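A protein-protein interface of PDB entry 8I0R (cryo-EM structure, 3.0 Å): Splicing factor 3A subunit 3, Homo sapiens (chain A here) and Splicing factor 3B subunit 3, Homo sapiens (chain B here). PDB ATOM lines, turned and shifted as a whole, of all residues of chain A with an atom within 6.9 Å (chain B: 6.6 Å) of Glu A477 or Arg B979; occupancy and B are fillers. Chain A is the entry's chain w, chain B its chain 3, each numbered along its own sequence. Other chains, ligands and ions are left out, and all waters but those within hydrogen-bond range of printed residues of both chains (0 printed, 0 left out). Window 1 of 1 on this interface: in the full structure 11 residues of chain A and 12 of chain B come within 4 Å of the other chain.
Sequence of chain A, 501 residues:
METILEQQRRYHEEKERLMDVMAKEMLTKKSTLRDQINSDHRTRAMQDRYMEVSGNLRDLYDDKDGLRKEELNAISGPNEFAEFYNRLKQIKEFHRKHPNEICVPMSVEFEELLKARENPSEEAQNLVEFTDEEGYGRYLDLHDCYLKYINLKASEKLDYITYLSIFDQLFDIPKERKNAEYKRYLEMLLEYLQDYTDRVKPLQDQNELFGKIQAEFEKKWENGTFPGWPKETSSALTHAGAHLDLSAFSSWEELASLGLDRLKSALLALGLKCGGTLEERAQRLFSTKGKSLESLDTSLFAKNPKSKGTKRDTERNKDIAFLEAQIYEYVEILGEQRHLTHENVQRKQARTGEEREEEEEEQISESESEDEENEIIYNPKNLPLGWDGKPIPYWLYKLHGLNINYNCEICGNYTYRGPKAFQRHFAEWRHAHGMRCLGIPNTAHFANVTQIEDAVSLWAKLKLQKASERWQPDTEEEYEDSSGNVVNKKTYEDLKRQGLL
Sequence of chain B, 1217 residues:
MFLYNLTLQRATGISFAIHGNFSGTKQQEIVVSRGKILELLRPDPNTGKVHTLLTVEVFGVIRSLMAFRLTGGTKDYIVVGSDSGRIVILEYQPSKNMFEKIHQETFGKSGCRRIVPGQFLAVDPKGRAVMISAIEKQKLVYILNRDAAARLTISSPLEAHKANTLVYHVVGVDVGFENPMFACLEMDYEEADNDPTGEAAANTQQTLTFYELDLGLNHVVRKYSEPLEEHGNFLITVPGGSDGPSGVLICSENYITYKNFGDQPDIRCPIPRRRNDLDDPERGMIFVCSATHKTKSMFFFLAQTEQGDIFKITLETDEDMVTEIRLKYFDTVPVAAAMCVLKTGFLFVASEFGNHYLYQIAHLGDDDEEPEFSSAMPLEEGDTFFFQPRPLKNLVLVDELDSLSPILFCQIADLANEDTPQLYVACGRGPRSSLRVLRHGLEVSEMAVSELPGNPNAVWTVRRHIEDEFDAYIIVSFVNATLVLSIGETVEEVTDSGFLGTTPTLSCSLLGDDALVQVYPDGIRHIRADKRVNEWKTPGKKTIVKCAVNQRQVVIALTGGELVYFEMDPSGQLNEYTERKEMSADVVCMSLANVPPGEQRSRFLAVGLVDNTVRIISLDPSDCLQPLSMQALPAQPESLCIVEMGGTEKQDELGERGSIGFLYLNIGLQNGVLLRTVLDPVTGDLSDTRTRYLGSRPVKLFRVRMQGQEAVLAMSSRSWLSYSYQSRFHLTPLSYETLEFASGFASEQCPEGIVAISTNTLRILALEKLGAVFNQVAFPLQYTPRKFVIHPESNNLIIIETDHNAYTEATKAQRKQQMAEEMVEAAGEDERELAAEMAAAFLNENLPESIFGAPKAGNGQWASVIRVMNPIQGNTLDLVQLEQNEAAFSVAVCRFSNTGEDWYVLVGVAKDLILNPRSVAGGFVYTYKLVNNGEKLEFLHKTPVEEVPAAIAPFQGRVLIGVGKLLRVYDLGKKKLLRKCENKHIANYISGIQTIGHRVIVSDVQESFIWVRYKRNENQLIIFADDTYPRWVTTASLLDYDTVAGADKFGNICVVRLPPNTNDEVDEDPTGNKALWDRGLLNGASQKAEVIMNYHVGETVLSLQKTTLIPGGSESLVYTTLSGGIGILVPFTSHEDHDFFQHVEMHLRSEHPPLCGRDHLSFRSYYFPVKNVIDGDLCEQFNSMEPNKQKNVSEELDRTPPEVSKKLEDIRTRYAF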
ATOM      1  N   TRP A 471     -14.398   7.559 -27.288  1.00  0.00           N
ATOM      2  CA  TRP A 471     -14.934   6.255 -26.926  1.00  0.00           C
ATOM      3  C   TRP A 471     -14.536   5.258 -28.002  1.00  0.00           C
ATOM      4  O   TRP A 471     -15.025   5.331 -29.133  1.00  0.00           O
ATOM      5  CB  TRP A 471     -16.451   6.350 -26.763  1.00  0.00           C
ATOM      6  CG  TRP A 471     -17.271   5.122 -27.008  1.00  0.00           C
ATOM      7  CD1 TRP A 471     -18.276   4.991 -27.915  1.00  0.00           C
ATOM      8  CD2 TRP A 471     -17.216   3.885 -26.296  1.00  0.00           C
ATOM      9  NE1 TRP A 471     -18.829   3.745 -27.835  1.00  0.00           N
ATOM     10  CE2 TRP A 471     -18.198   3.046 -26.844  1.00  0.00           C
ATOM     11  CE3 TRP A 471     -16.426   3.399 -25.256  1.00  0.00           C
ATOM     12  CZ2 TRP A 471     -18.406   1.755 -26.394  1.00  0.00           C
ATOM     13  CZ3 TRP A 471     -16.637   2.118 -24.818  1.00  0.00           C
ATOM     14  CH2 TRP A 471     -17.619   1.314 -25.378  1.00  0.00           C
ATOM     15  N   GLN A 472     -13.635   4.346 -27.655  1.00  0.00           N
ATOM     16  CA  GLN A 472     -13.190   3.308 -28.576  1.00  0.00           C
ATOM     17  C   GLN A 472     -13.823   1.986 -28.177  1.00  0.00           C
ATOM     18  O   GLN A 472     -13.405   1.387 -27.176  1.00  0.00           O
ATOM     19  CB  GLN A 472     -11.667   3.183 -28.584  1.00  0.00           C
ATOM     20  CG  GLN A 472     -10.979   3.537 -27.285  1.00  0.00           C
ATOM     21  CD  GLN A 472     -10.900   5.024 -27.057  1.00  0.00           C
ATOM     22  OE1 GLN A 472     -10.496   5.778 -27.940  1.00  0.00           O
ATOM     23  NE2 GLN A 472     -11.291   5.458 -25.870  1.00  0.00           N
ATOM     24  N   PRO A 473     -14.813   1.495 -28.907  1.00  0.00           N
ATOM     25  CA  PRO A 473     -15.427   0.220 -28.539  1.00  0.00           C
ATOM     26  C   PRO A 473     -14.423  -0.914 -28.595  1.00  0.00           C
ATOM     27  O   PRO A 473     -14.427  -1.807 -27.743  1.00  0.00           O
ATOM     28  CB  PRO A 473     -16.536   0.047 -29.583  1.00  0.00           C
ATOM     29  CG  PRO A 473     -16.758   1.399 -30.137  1.00  0.00           C
ATOM     30  CD  PRO A 473     -15.444   2.086 -30.094  1.00  0.00           C
ATOM     31  N   ASP A 474     -13.545  -0.864 -29.593  1.00  0.00           N
ATOM     32  CA  ASP A 474     -12.547  -1.896 -29.840  1.00  0.00           C
ATOM     33  C   ASP A 474     -11.736  -2.246 -28.600  1.00  0.00           C
ATOM     34  O   ASP A 474     -11.356  -3.405 -28.409  1.00  0.00           O
ATOM     35  CB  ASP A 474     -11.609  -1.448 -30.959  1.00  0.00           C
ATOM     36  CG  ASP A 474     -12.358  -0.892 -32.146  1.00  0.00           C
ATOM     37  OD1 ASP A 474     -13.542  -1.246 -32.308  1.00  0.00           O
ATOM     38  OD2 ASP A 474     -11.777  -0.093 -32.909  1.00  0.00           O
ATOM     39  N   THR A 475     -11.472  -1.263 -27.748  1.00  0.00           N
ATOM     40  CA  THR A 475     -10.590  -1.471 -26.615  1.00  0.00           C
ATOM     41  C   THR A 475     -11.315  -1.671 -25.298  1.00  0.00           C
ATOM     42  O   THR A 475     -10.874  -2.483 -24.488  1.00  0.00           O
ATOM     43  CB  THR A 475      -9.636  -0.286 -26.467  1.00  0.00           C
ATOM     44  OG1 THR A 475     -10.314   0.781 -25.797  1.00  0.00           O
ATOM     45  CG2 THR A 475      -9.184   0.185 -27.834  1.00  0.00           C
ATOM     46  N   GLU A 476     -12.415  -0.968 -25.065  1.00  0.00           N
ATOM     47  CA  GLU A 476     -13.169  -1.159 -23.841  1.00  0.00           C
ATOM     48  C   GLU A 476     -14.195  -2.272 -23.927  1.00  0.00           C
ATOM     49  O   GLU A 476     -14.150  -3.181 -23.097  1.00  0.00           O
ATOM     50  CB  GLU A 476     -13.877   0.133 -23.419  1.00  0.00           C
ATOM     51  CG  GLU A 476     -12.987   1.345 -23.396  1.00  0.00           C
ATOM     52  CD  GLU A 476     -13.773   2.602 -23.158  1.00  0.00           C
ATOM     53  OE1 GLU A 476     -13.291   3.693 -23.526  1.00  0.00           O
ATOM     54  OE2 GLU A 476     -14.869   2.494 -22.576  1.00  0.00           O
ATOM     55  N   GLU A 477     -15.095  -2.234 -24.908  1.00  0.00           N
ATOM     56  CA  GLU A 477     -16.276  -3.088 -24.901  1.00  0.00           C
ATOM     57  C   GLU A 477     -15.867  -4.524 -24.611  1.00  0.00           C
ATOM     58  O   GLU A 477     -15.295  -5.194 -25.474  1.00  0.00           O
ATOM     59  CB  GLU A 477     -16.992  -2.990 -26.241  1.00  0.00           C
ATOM     60  CG  GLU A 477     -18.270  -3.792 -26.341  1.00  0.00           C
ATOM     61  CD  GLU A 477     -19.202  -3.246 -27.409  1.00  0.00           C
ATOM     62  OE1 GLU A 477     -20.319  -3.776 -27.566  1.00  0.00           O
ATOM     63  OE2 GLU A 477     -18.811  -2.286 -28.104  1.00  0.00           O
ATOM     64  N   GLU A 478     -16.153  -4.992 -23.396  1.00  0.00           N
ATOM     65  CA  GLU A 478     -15.626  -6.265 -22.927  1.00  0.00           C
ATOM     66  C   GLU A 478     -16.637  -7.378 -23.149  1.00  0.00           C
ATOM     67  O   GLU A 478     -17.783  -7.286 -22.705  1.00  0.00           O
ATOM     68  CB  GLU A 478     -15.217  -6.196 -21.455  1.00  0.00           C
ATOM     69  CG  GLU A 478     -16.221  -5.588 -20.494  1.00  0.00           C
ATOM     70  CD  GLU A 478     -15.548  -4.881 -19.310  1.00  0.00           C
ATOM     71  OE1 GLU A 478     -14.341  -5.109 -19.083  1.00  0.00           O
ATOM     72  OE2 GLU A 478     -16.232  -4.130 -18.581  1.00  0.00           O
ATOM     73  N   TYR A 479     -16.185  -8.434 -23.820  1.00  0.00           N
ATOM     74  CA  TYR A 479     -17.013  -9.538 -24.283  1.00  0.00           C
ATOM     75  C   TYR A 479     -16.598 -10.827 -23.593  1.00  0.00           C
ATOM     76  O   TYR A 479     -15.425 -11.204 -23.613  1.00  0.00           O
ATOM     77  CB  TYR A 479     -16.869  -9.721 -25.784  1.00  0.00           C
ATOM     78  CG  TYR A 479     -17.941  -9.051 -26.580  1.00  0.00           C
ATOM     79  CD1 TYR A 479     -18.990  -9.780 -27.104  1.00  0.00           C
ATOM     80  CD2 TYR A 479     -17.908  -7.688 -26.813  1.00  0.00           C
ATOM     81  CE1 TYR A 479     -19.978  -9.174 -27.835  1.00  0.00           C
ATOM     82  CE2 TYR A 479     -18.895  -7.071 -27.541  1.00  0.00           C
ATOM     83  CZ  TYR A 479     -19.925  -7.820 -28.056  1.00  0.00           C
ATOM     84  OH  TYR A 479     -20.913  -7.211 -28.786  1.00  0.00           O
ATOM     85  N   VAL A 487     -13.157 -11.196 -23.272  1.00  0.00           N
ATOM     86  CA  VAL A 487     -12.293 -10.624 -24.291  1.00  0.00           C
ATOM     87  C   VAL A 487     -12.887  -9.278 -24.677  1.00  0.00           C
ATOM     88  O   VAL A 487     -14.049  -8.991 -24.393  1.00  0.00           O
ATOM     89  CB  VAL A 487     -12.170 -11.531 -25.529  1.00  0.00           C
ATOM     90  CG1 VAL A 487     -11.747 -12.923 -25.128  1.00  0.00           C
ATOM     91  CG2 VAL A 487     -13.485 -11.586 -26.270  1.00  0.00           C
ATOM     92  N   ASN A 488     -12.086  -8.437 -25.318  1.00  0.00           N
ATOM     93  CA  ASN A 488     -12.702  -7.288 -25.960  1.00  0.00           C
ATOM     94  C   ASN A 488     -13.312  -7.723 -27.288  1.00  0.00           C
ATOM     95  O   ASN A 488     -12.988  -8.786 -27.823  1.00  0.00           O
ATOM     96  CB  ASN A 488     -11.696  -6.156 -26.160  1.00  0.00           C
ATOM     97  CG  ASN A 488     -10.473  -6.590 -26.926  1.00  0.00           C
ATOM     98  OD1 ASN A 488     -10.564  -7.025 -28.071  1.00  0.00           O
ATOM     99  ND2 ASN A 488      -9.312  -6.464 -26.299  1.00  0.00           N
ATOM    100  N   LYS A 489     -14.211  -6.897 -27.823  1.00  0.00           N
ATOM    101  CA  LYS A 489     -14.958  -7.321 -29.002  1.00  0.00           C
ATOM    102  C   LYS A 489     -14.037  -7.541 -30.193  1.00  0.00           C
ATOM    103  O   LYS A 489     -14.360  -8.315 -31.100  1.00  0.00           O
ATOM    104  CB  LYS A 489     -16.043  -6.309 -29.357  1.00  0.00           C
ATOM    105  CG  LYS A 489     -17.048  -6.871 -30.346  1.00  0.00           C
ATOM    106  CD  LYS A 489     -17.158  -6.032 -31.592  1.00  0.00           C
ATOM    107  CE  LYS A 489     -18.463  -6.316 -32.300  1.00  0.00           C
ATOM    108  NZ  LYS A 489     -19.620  -6.016 -31.420  1.00  0.00           N
ATOM    109  N   LYS A 490     -12.882  -6.872 -30.206  1.00  0.00           N
ATOM    110  CA  LYS A 490     -11.922  -7.102 -31.277  1.00  0.00           C
ATOM    111  C   LYS A 490     -11.543  -8.574 -31.357  1.00  0.00           C
ATOM    112  O   LYS A 490     -11.854  -9.250 -32.342  1.00  0.00           O
ATOM    113  CB  LYS A 490     -10.680  -6.238 -31.069  1.00  0.00           C
ATOM    114  CG  LYS A 490      -9.850  -6.039 -32.326  1.00  0.00           C
ATOM    115  CD  LYS A 490      -8.811  -4.957 -32.125  1.00  0.00           C
ATOM    116  CE  LYS A 490      -7.910  -5.281 -30.955  1.00  0.00           C
ATOM    117  NZ  LYS A 490      -6.830  -4.280 -30.816  1.00  0.00           N
ATOM    118  N   TYR A 492     -12.919 -10.889 -29.818  1.00  0.00           N
ATOM    119  CA  TYR A 492     -14.160 -11.648 -29.907  1.00  0.00           C
ATOM    120  C   TYR A 492     -14.479 -11.988 -31.350  1.00  0.00           C
ATOM    121  O   TYR A 492     -14.639 -13.158 -31.703  1.00  0.00           O
ATOM    122  CB  TYR A 492     -15.315 -10.866 -29.292  1.00  0.00           C
ATOM    123  CG  TYR A 492     -16.669 -11.375 -29.733  1.00  0.00           C
ATOM    124  CD1 TYR A 492     -17.556 -10.552 -30.409  1.00  0.00           C
ATOM    125  CD2 TYR A 492     -17.059 -12.681 -29.470  1.00  0.00           C
ATOM    126  CE1 TYR A 492     -18.788 -11.017 -30.814  1.00  0.00           C
ATOM    127  CE2 TYR A 492     -18.292 -13.152 -29.871  1.00  0.00           C
ATOM    128  CZ  TYR A 492     -19.150 -12.315 -30.542  1.00  0.00           C
ATOM    129  OH  TYR A 492     -20.379 -12.773 -30.942  1.00  0.00           O
ATOM    130  N   GLU B 946     -14.336   1.260 -10.577  1.00  0.00           N
ATOM    131  CA  GLU B 946     -13.272   2.157 -10.142  1.00  0.00           C
ATOM    132  C   GLU B 946     -13.744   3.311  -9.261  1.00  0.00           C
ATOM    133  O   GLU B 946     -12.915   4.131  -8.857  1.00  0.00           O
ATOM    134  CB  GLU B 946     -12.521   2.719 -11.348  1.00  0.00           C
ATOM    135  CG  GLU B 946     -13.397   3.181 -12.492  1.00  0.00           C
ATOM    136  CD  GLU B 946     -13.824   2.041 -13.388  1.00  0.00           C
ATOM    137  OE1 GLU B 946     -14.085   0.936 -12.868  1.00  0.00           O
ATOM    138  OE2 GLU B 946     -13.874   2.242 -14.615  1.00  0.00           O
ATOM    139  N   ARG B 958     -30.933  -3.662 -20.761  1.00  0.00           N
ATOM    140  CA  ARG B 958     -29.610  -3.622 -20.169  1.00  0.00           C
ATOM    141  C   ARG B 958     -29.668  -2.638 -19.011  1.00  0.00           C
ATOM    142  O   ARG B 958     -30.749  -2.234 -18.588  1.00  0.00           O
ATOM    143  CB  ARG B 958     -28.558  -3.256 -21.217  1.00  0.00           C
ATOM    144  CG  ARG B 958     -29.099  -3.327 -22.640  1.00  0.00           C
ATOM    145  CD  ARG B 958     -28.090  -3.858 -23.625  1.00  0.00           C
ATOM    146  NE  ARG B 958     -27.510  -2.816 -24.459  1.00  0.00           N
ATOM    147  CZ  ARG B 958     -26.425  -2.988 -25.200  1.00  0.00           C
ATOM    148  NH1 ARG B 958     -25.821  -4.163 -25.217  1.00  0.00           N
ATOM    149  NH2 ARG B 958     -25.952  -1.993 -25.930  1.00  0.00           N
ATOM    150  N   ARG B 968     -21.855   4.428 -17.838  1.00  0.00           N
ATOM    151  CA  ARG B 968     -21.627   3.239 -18.631  1.00  0.00           C
ATOM    152  C   ARG B 968     -22.922   2.481 -18.826  1.00  0.00           C
ATOM    153  O   ARG B 968     -23.826   2.546 -18.002  1.00  0.00           O
ATOM    154  CB  ARG B 968     -20.597   2.346 -17.967  1.00  0.00           C
ATOM    155  CG  ARG B 968     -19.316   3.071 -17.754  1.00  0.00           C
ATOM    156  CD  ARG B 968     -18.392   2.332 -16.867  1.00  0.00           C
ATOM    157  NE  ARG B 968     -17.027   2.597 -17.264  1.00  0.00           N
ATOM    158  CZ  ARG B 968     -15.979   2.313 -16.512  1.00  0.00           C
ATOM    159  NH1 ARG B 968     -16.152   1.757 -15.329  1.00  0.00           N
ATOM    160  NH2 ARG B 968     -14.759   2.589 -16.940  1.00  0.00           N
ATOM    161  N   VAL B 969     -23.017   1.784 -19.942  1.00  0.00           N
ATOM    162  CA  VAL B 969     -24.115   0.870 -20.194  1.00  0.00           C
ATOM    163  C   VAL B 969     -23.543  -0.521 -20.078  1.00  0.00           C
ATOM    164  O   VAL B 969     -22.564  -0.839 -20.756  1.00  0.00           O
ATOM    165  CB  VAL B 969     -24.736   1.084 -21.577  1.00  0.00           C
ATOM    166  CG1 VAL B 969     -25.597  -0.097 -21.932  1.00  0.00           C
ATOM    167  CG2 VAL B 969     -25.546   2.328 -21.583  1.00  0.00           C
ATOM    168  N   TYR B 970     -24.120  -1.328 -19.202  1.00  0.00           N
ATOM    169  CA  TYR B 970     -23.696  -2.685 -18.937  1.00  0.00           C
ATOM    170  C   TYR B 970     -24.751  -3.657 -19.429  1.00  0.00           C
ATOM    171  O   TYR B 970     -25.947  -3.351 -19.486  1.00  0.00           O
ATOM    172  CB  TYR B 970     -23.473  -2.917 -17.446  1.00  0.00           C
ATOM    173  CG  TYR B 970     -22.184  -2.374 -16.897  1.00  0.00           C
ATOM    174  CD1 TYR B 970     -21.141  -3.209 -16.600  1.00  0.00           C
ATOM    175  CD2 TYR B 970     -22.027  -1.034 -16.643  1.00  0.00           C
ATOM    176  CE1 TYR B 970     -19.971  -2.727 -16.094  1.00  0.00           C
ATOM    177  CE2 TYR B 970     -20.861  -0.544 -16.137  1.00  0.00           C
ATOM    178  CZ  TYR B 970     -19.838  -1.397 -15.863  1.00  0.00           C
ATOM    179  OH  TYR B 970     -18.666  -0.912 -15.355  1.00  0.00           O
ATOM    180  N   ASP B 971     -24.279  -4.851 -19.762  1.00  0.00           N
ATOM    181  CA  ASP B 971     -25.149  -5.975 -20.038  1.00  0.00           C
ATOM    182  C   ASP B 971     -24.683  -7.163 -19.216  1.00  0.00           C
ATOM    183  O   ASP B 971     -23.585  -7.167 -18.653  1.00  0.00           O
ATOM    184  CB  ASP B 971     -25.185  -6.340 -21.520  1.00  0.00           C
ATOM    185  CG  ASP B 971     -26.450  -7.086 -21.899  1.00  0.00           C
ATOM    186  OD1 ASP B 971     -27.039  -7.745 -21.022  1.00  0.00           O
ATOM    187  OD2 ASP B 971     -26.859  -7.016 -23.073  1.00  0.00           O
ATOM    188  N   LYS B 976     -19.197 -11.913 -14.843  1.00  0.00           N
ATOM    189  CA  LYS B 976     -19.265 -10.554 -14.329  1.00  0.00           C
ATOM    190  C   LYS B 976     -20.018  -9.710 -15.341  1.00  0.00           C
ATOM    191  O   LYS B 976     -20.350 -10.176 -16.431  1.00  0.00           O
ATOM    192  CB  LYS B 976     -17.878  -9.980 -14.073  1.00  0.00           C
ATOM    193  CG  LYS B 976     -17.187  -9.536 -15.327  1.00  0.00           C
ATOM    194  CD  LYS B 976     -15.817  -9.006 -15.006  1.00  0.00           C
ATOM    195  CE  LYS B 976     -15.326  -8.123 -16.115  1.00  0.00           C
ATOM    196  NZ  LYS B 976     -15.559  -8.777 -17.420  1.00  0.00           N
ATOM    197  N   LEU B 977     -20.279  -8.459 -14.972  1.00  0.00           N
ATOM    198  CA  LEU B 977     -21.029  -7.570 -15.845  1.00  0.00           C
ATOM    199  C   LEU B 977     -20.138  -7.031 -16.958  1.00  0.00           C
ATOM    200  O   LEU B 977     -18.950  -6.774 -16.759  1.00  0.00           O
ATOM    201  CB  LEU B 977     -21.614  -6.420 -15.032  1.00  0.00           C
ATOM    202  CG  LEU B 977     -22.945  -6.676 -14.336  1.00  0.00           C
ATOM    203  CD1 LEU B 977     -23.300  -5.482 -13.503  1.00  0.00           C
ATOM    204  CD2 LEU B 977     -24.015  -6.938 -15.352  1.00  0.00           C
ATOM    205  N   LEU B 978     -20.720  -6.836 -18.138  1.00  0.00           N
ATOM    206  CA  LEU B 978     -19.957  -6.447 -19.308  1.00  0.00           C
ATOM    207  C   LEU B 978     -20.256  -5.002 -19.676  1.00  0.00           C
ATOM    208  O   LEU B 978     -21.399  -4.554 -19.619  1.00  0.00           O
ATOM    209  CB  LEU B 978     -20.276  -7.356 -20.495  1.00  0.00           C
ATOM    210  CG  LEU B 978     -20.376  -8.853 -20.219  1.00  0.00           C
ATOM    211  CD1 LEU B 978     -20.526  -9.595 -21.521  1.00  0.00           C
ATOM    212  CD2 LEU B 978     -19.159  -9.344 -19.472  1.00  0.00           C
ATOM    213  N   ARG B 979     -19.214  -4.290 -20.092  1.00  0.00           N
ATOM    214  CA  ARG B 979     -19.287  -2.868 -20.411  1.00  0.00           C
ATOM    215  C   ARG B 979     -19.595  -2.708 -21.892  1.00  0.00           C
ATOM    216  O   ARG B 979     -18.701  -2.797 -22.735  1.00  0.00           O
ATOM    217  CB  ARG B 979     -17.979  -2.177 -20.054  1.00  0.00           C
ATOM    218  CG  ARG B 979     -17.715  -0.896 -20.788  1.00  0.00           C
ATOM    219  CD  ARG B 979     -16.970   0.054 -19.912  1.00  0.00           C
ATOM    220  NE  ARG B 979     -15.541  -0.186 -19.976  1.00  0.00           N
ATOM    221  CZ  ARG B 979     -14.889  -0.986 -19.149  1.00  0.00           C
ATOM    222  NH1 ARG B 979     -15.543  -1.623 -18.191  1.00  0.00           N
ATOM    223  NH2 ARG B 979     -13.582  -1.151 -19.277  1.00  0.00           N
ATOM    224  N   LYS B 980     -20.855  -2.480 -22.206  1.00  0.00           N
ATOM    225  CA  LYS B 980     -21.297  -2.339 -23.571  1.00  0.00           C
ATOM    226  C   LYS B 980     -21.202  -0.917 -24.101  1.00  0.00           C
ATOM    227  O   LYS B 980     -21.203  -0.735 -25.320  1.00  0.00           O
ATOM    228  CB  LYS B 980     -22.737  -2.821 -23.690  1.00  0.00           C
ATOM    229  CG  LYS B 980     -22.841  -4.184 -24.301  1.00  0.00           C
ATOM    230  CD  LYS B 980     -21.964  -5.179 -23.579  1.00  0.00           C
ATOM    231  CE  LYS B 980     -21.443  -6.208 -24.545  1.00  0.00           C
ATOM    232  NZ  LYS B 980     -22.561  -6.835 -25.300  1.00  0.00           N
ATOM    233  N   CYS B 981     -21.130   0.094 -23.240  1.00  0.00           N
ATOM    234  CA  CYS B 981     -20.969   1.458 -23.739  1.00  0.00           C
ATOM    235  C   CYS B 981     -20.533   2.350 -22.594  1.00  0.00           C
ATOM    236  O   CYS B 981     -20.547   1.943 -21.433  1.00  0.00           O
ATOM    237  CB  CYS B 981     -22.249   2.007 -24.363  1.00  0.00           C
ATOM    238  SG  CYS B 981     -21.959   3.450 -25.384  1.00  0.00           S
ATOM    239  N   GLU B 982     -20.210   3.595 -22.926  1.00  0.00           N
ATOM    240  CA  GLU B 982     -19.688   4.502 -21.923  1.00  0.00           C
ATOM    241  C   GLU B 982     -19.650   5.908 -22.480  1.00  0.00           C
ATOM    242  O   GLU B 982     -19.383   6.117 -23.660  1.00  0.00           O
ATOM    243  CB  GLU B 982     -18.294   4.077 -21.479  1.00  0.00           C
ATOM    244  CG  GLU B 982     -17.388   5.204 -21.089  1.00  0.00           C
ATOM    245  CD  GLU B 982     -16.491   4.830 -19.944  1.00  0.00           C
ATOM    246  OE1 GLU B 982     -16.671   3.740 -19.374  1.00  0.00           O
ATOM    247  OE2 GLU B 982     -15.587   5.612 -19.621  1.00  0.00           O
ATOM    248  N   ASN B1019     -24.618   2.705 -31.300  1.00  0.00           N
ATOM    249  CA  ASN B1019     -24.109   2.384 -29.969  1.00  0.00           C
ATOM    250  C   ASN B1019     -23.369   3.567 -29.348  1.00  0.00           C
ATOM    251  O   ASN B1019     -22.166   3.508 -29.093  1.00  0.00           O
ATOM    252  CB  ASN B1019     -23.216   1.146 -30.021  1.00  0.00           C
ATOM    253  CG  ASN B1019     -22.725   0.723 -28.657  1.00  0.00           C
ATOM    254  OD1 ASN B1019     -23.263  -0.202 -28.055  1.00  0.00           O
ATOM    255  ND2 ASN B1019     -21.693   1.396 -28.162  1.00  0.00           N
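The guanidinium group (NE) of Arg B979 lies within salt-bridge range of the side-chain carboxylate (OE2) of Glu A476, 3.8 Å away. NH1 of Arg B979 lies within salt-bridge range of OE2 of Glu A478 (2.6 Å).
Of the 14 printed residues of chain A, 5 touch a printed residue of chain B. Hydrophobic or aromatic side chains of chain A that line the printed part of chain B: Trp A471 and Tyr A479. Printed residues of chain B that touch a printed residue of chain A: Leu B978, Arg B979, Lys B980, Cys B981, Glu B982 and Asn B1019. Hydrophobic or aromatic side chains of chain B within 4 Å of the printed part of chain A: Leu B978. Among the printed residues, Asp or Glu carboxylates within 4 Å of a Lys or Arg side-chain nitrogen of the other chain: Glu A476 with Arg B979 and Glu A478 with Arg B979.
Asp A474 touches none of the printed residues of chain B. Glu A477 touches just these residues of chain B: Arg B979 and Lys B980. Printed residues of chain B within 4 Å of Tyr A479: Lys B980. Tyr B970 touches none of the printed residues of chain A. Arg B979 touches three residues of chain A. Of the printed residues of chain A, Lys B980 touches Trp A471 (3.9 Å), Glu A477 (3.8 Å) and Tyr A479 (3.9 Å). The nearest residue of chain B that does not touch Glu A477 is Asn B1019 (4.7 Å). The nearest printed residue of chain A that does not touch Asn B1019 is Glu A477 (4.7 Å).
Among the printed residues, merely in contact across the chains: Trp A471 with Lys B980, Trp A471 with Cys B981, Trp A471 with Asn B1019, Glu A476 with Glu B982, Glu A477 with Arg B979, Glu A477 with Lys B980, Glu A478 with Leu B978 and Tyr A479 with Lys B980.
The guanidinium group of Arg B968 is in salt-bridge range of the side-chain carboxylate of Glu B982 (2.4 Å). N of Lys B980 lies within hydrogen-bond range of O of Val B969 (2.8 Å). N of Asp B971 lies within hydrogen-bond range of O of Leu B978 (2.9 Å). The side-chain sulfur (SG) of Cys B981 is in hydrogen-bond range of the side-chain amide nitrogen (ND2) of Asn B1019, 3.5 Å away. The backbone carbonyl oxygen (O) of Glu A477 sits at hydrogen-bond distance from the backbone NH (N) of Lys A489. O of Tyr A479 lies close to O of Val A487, 2.7 Å away.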
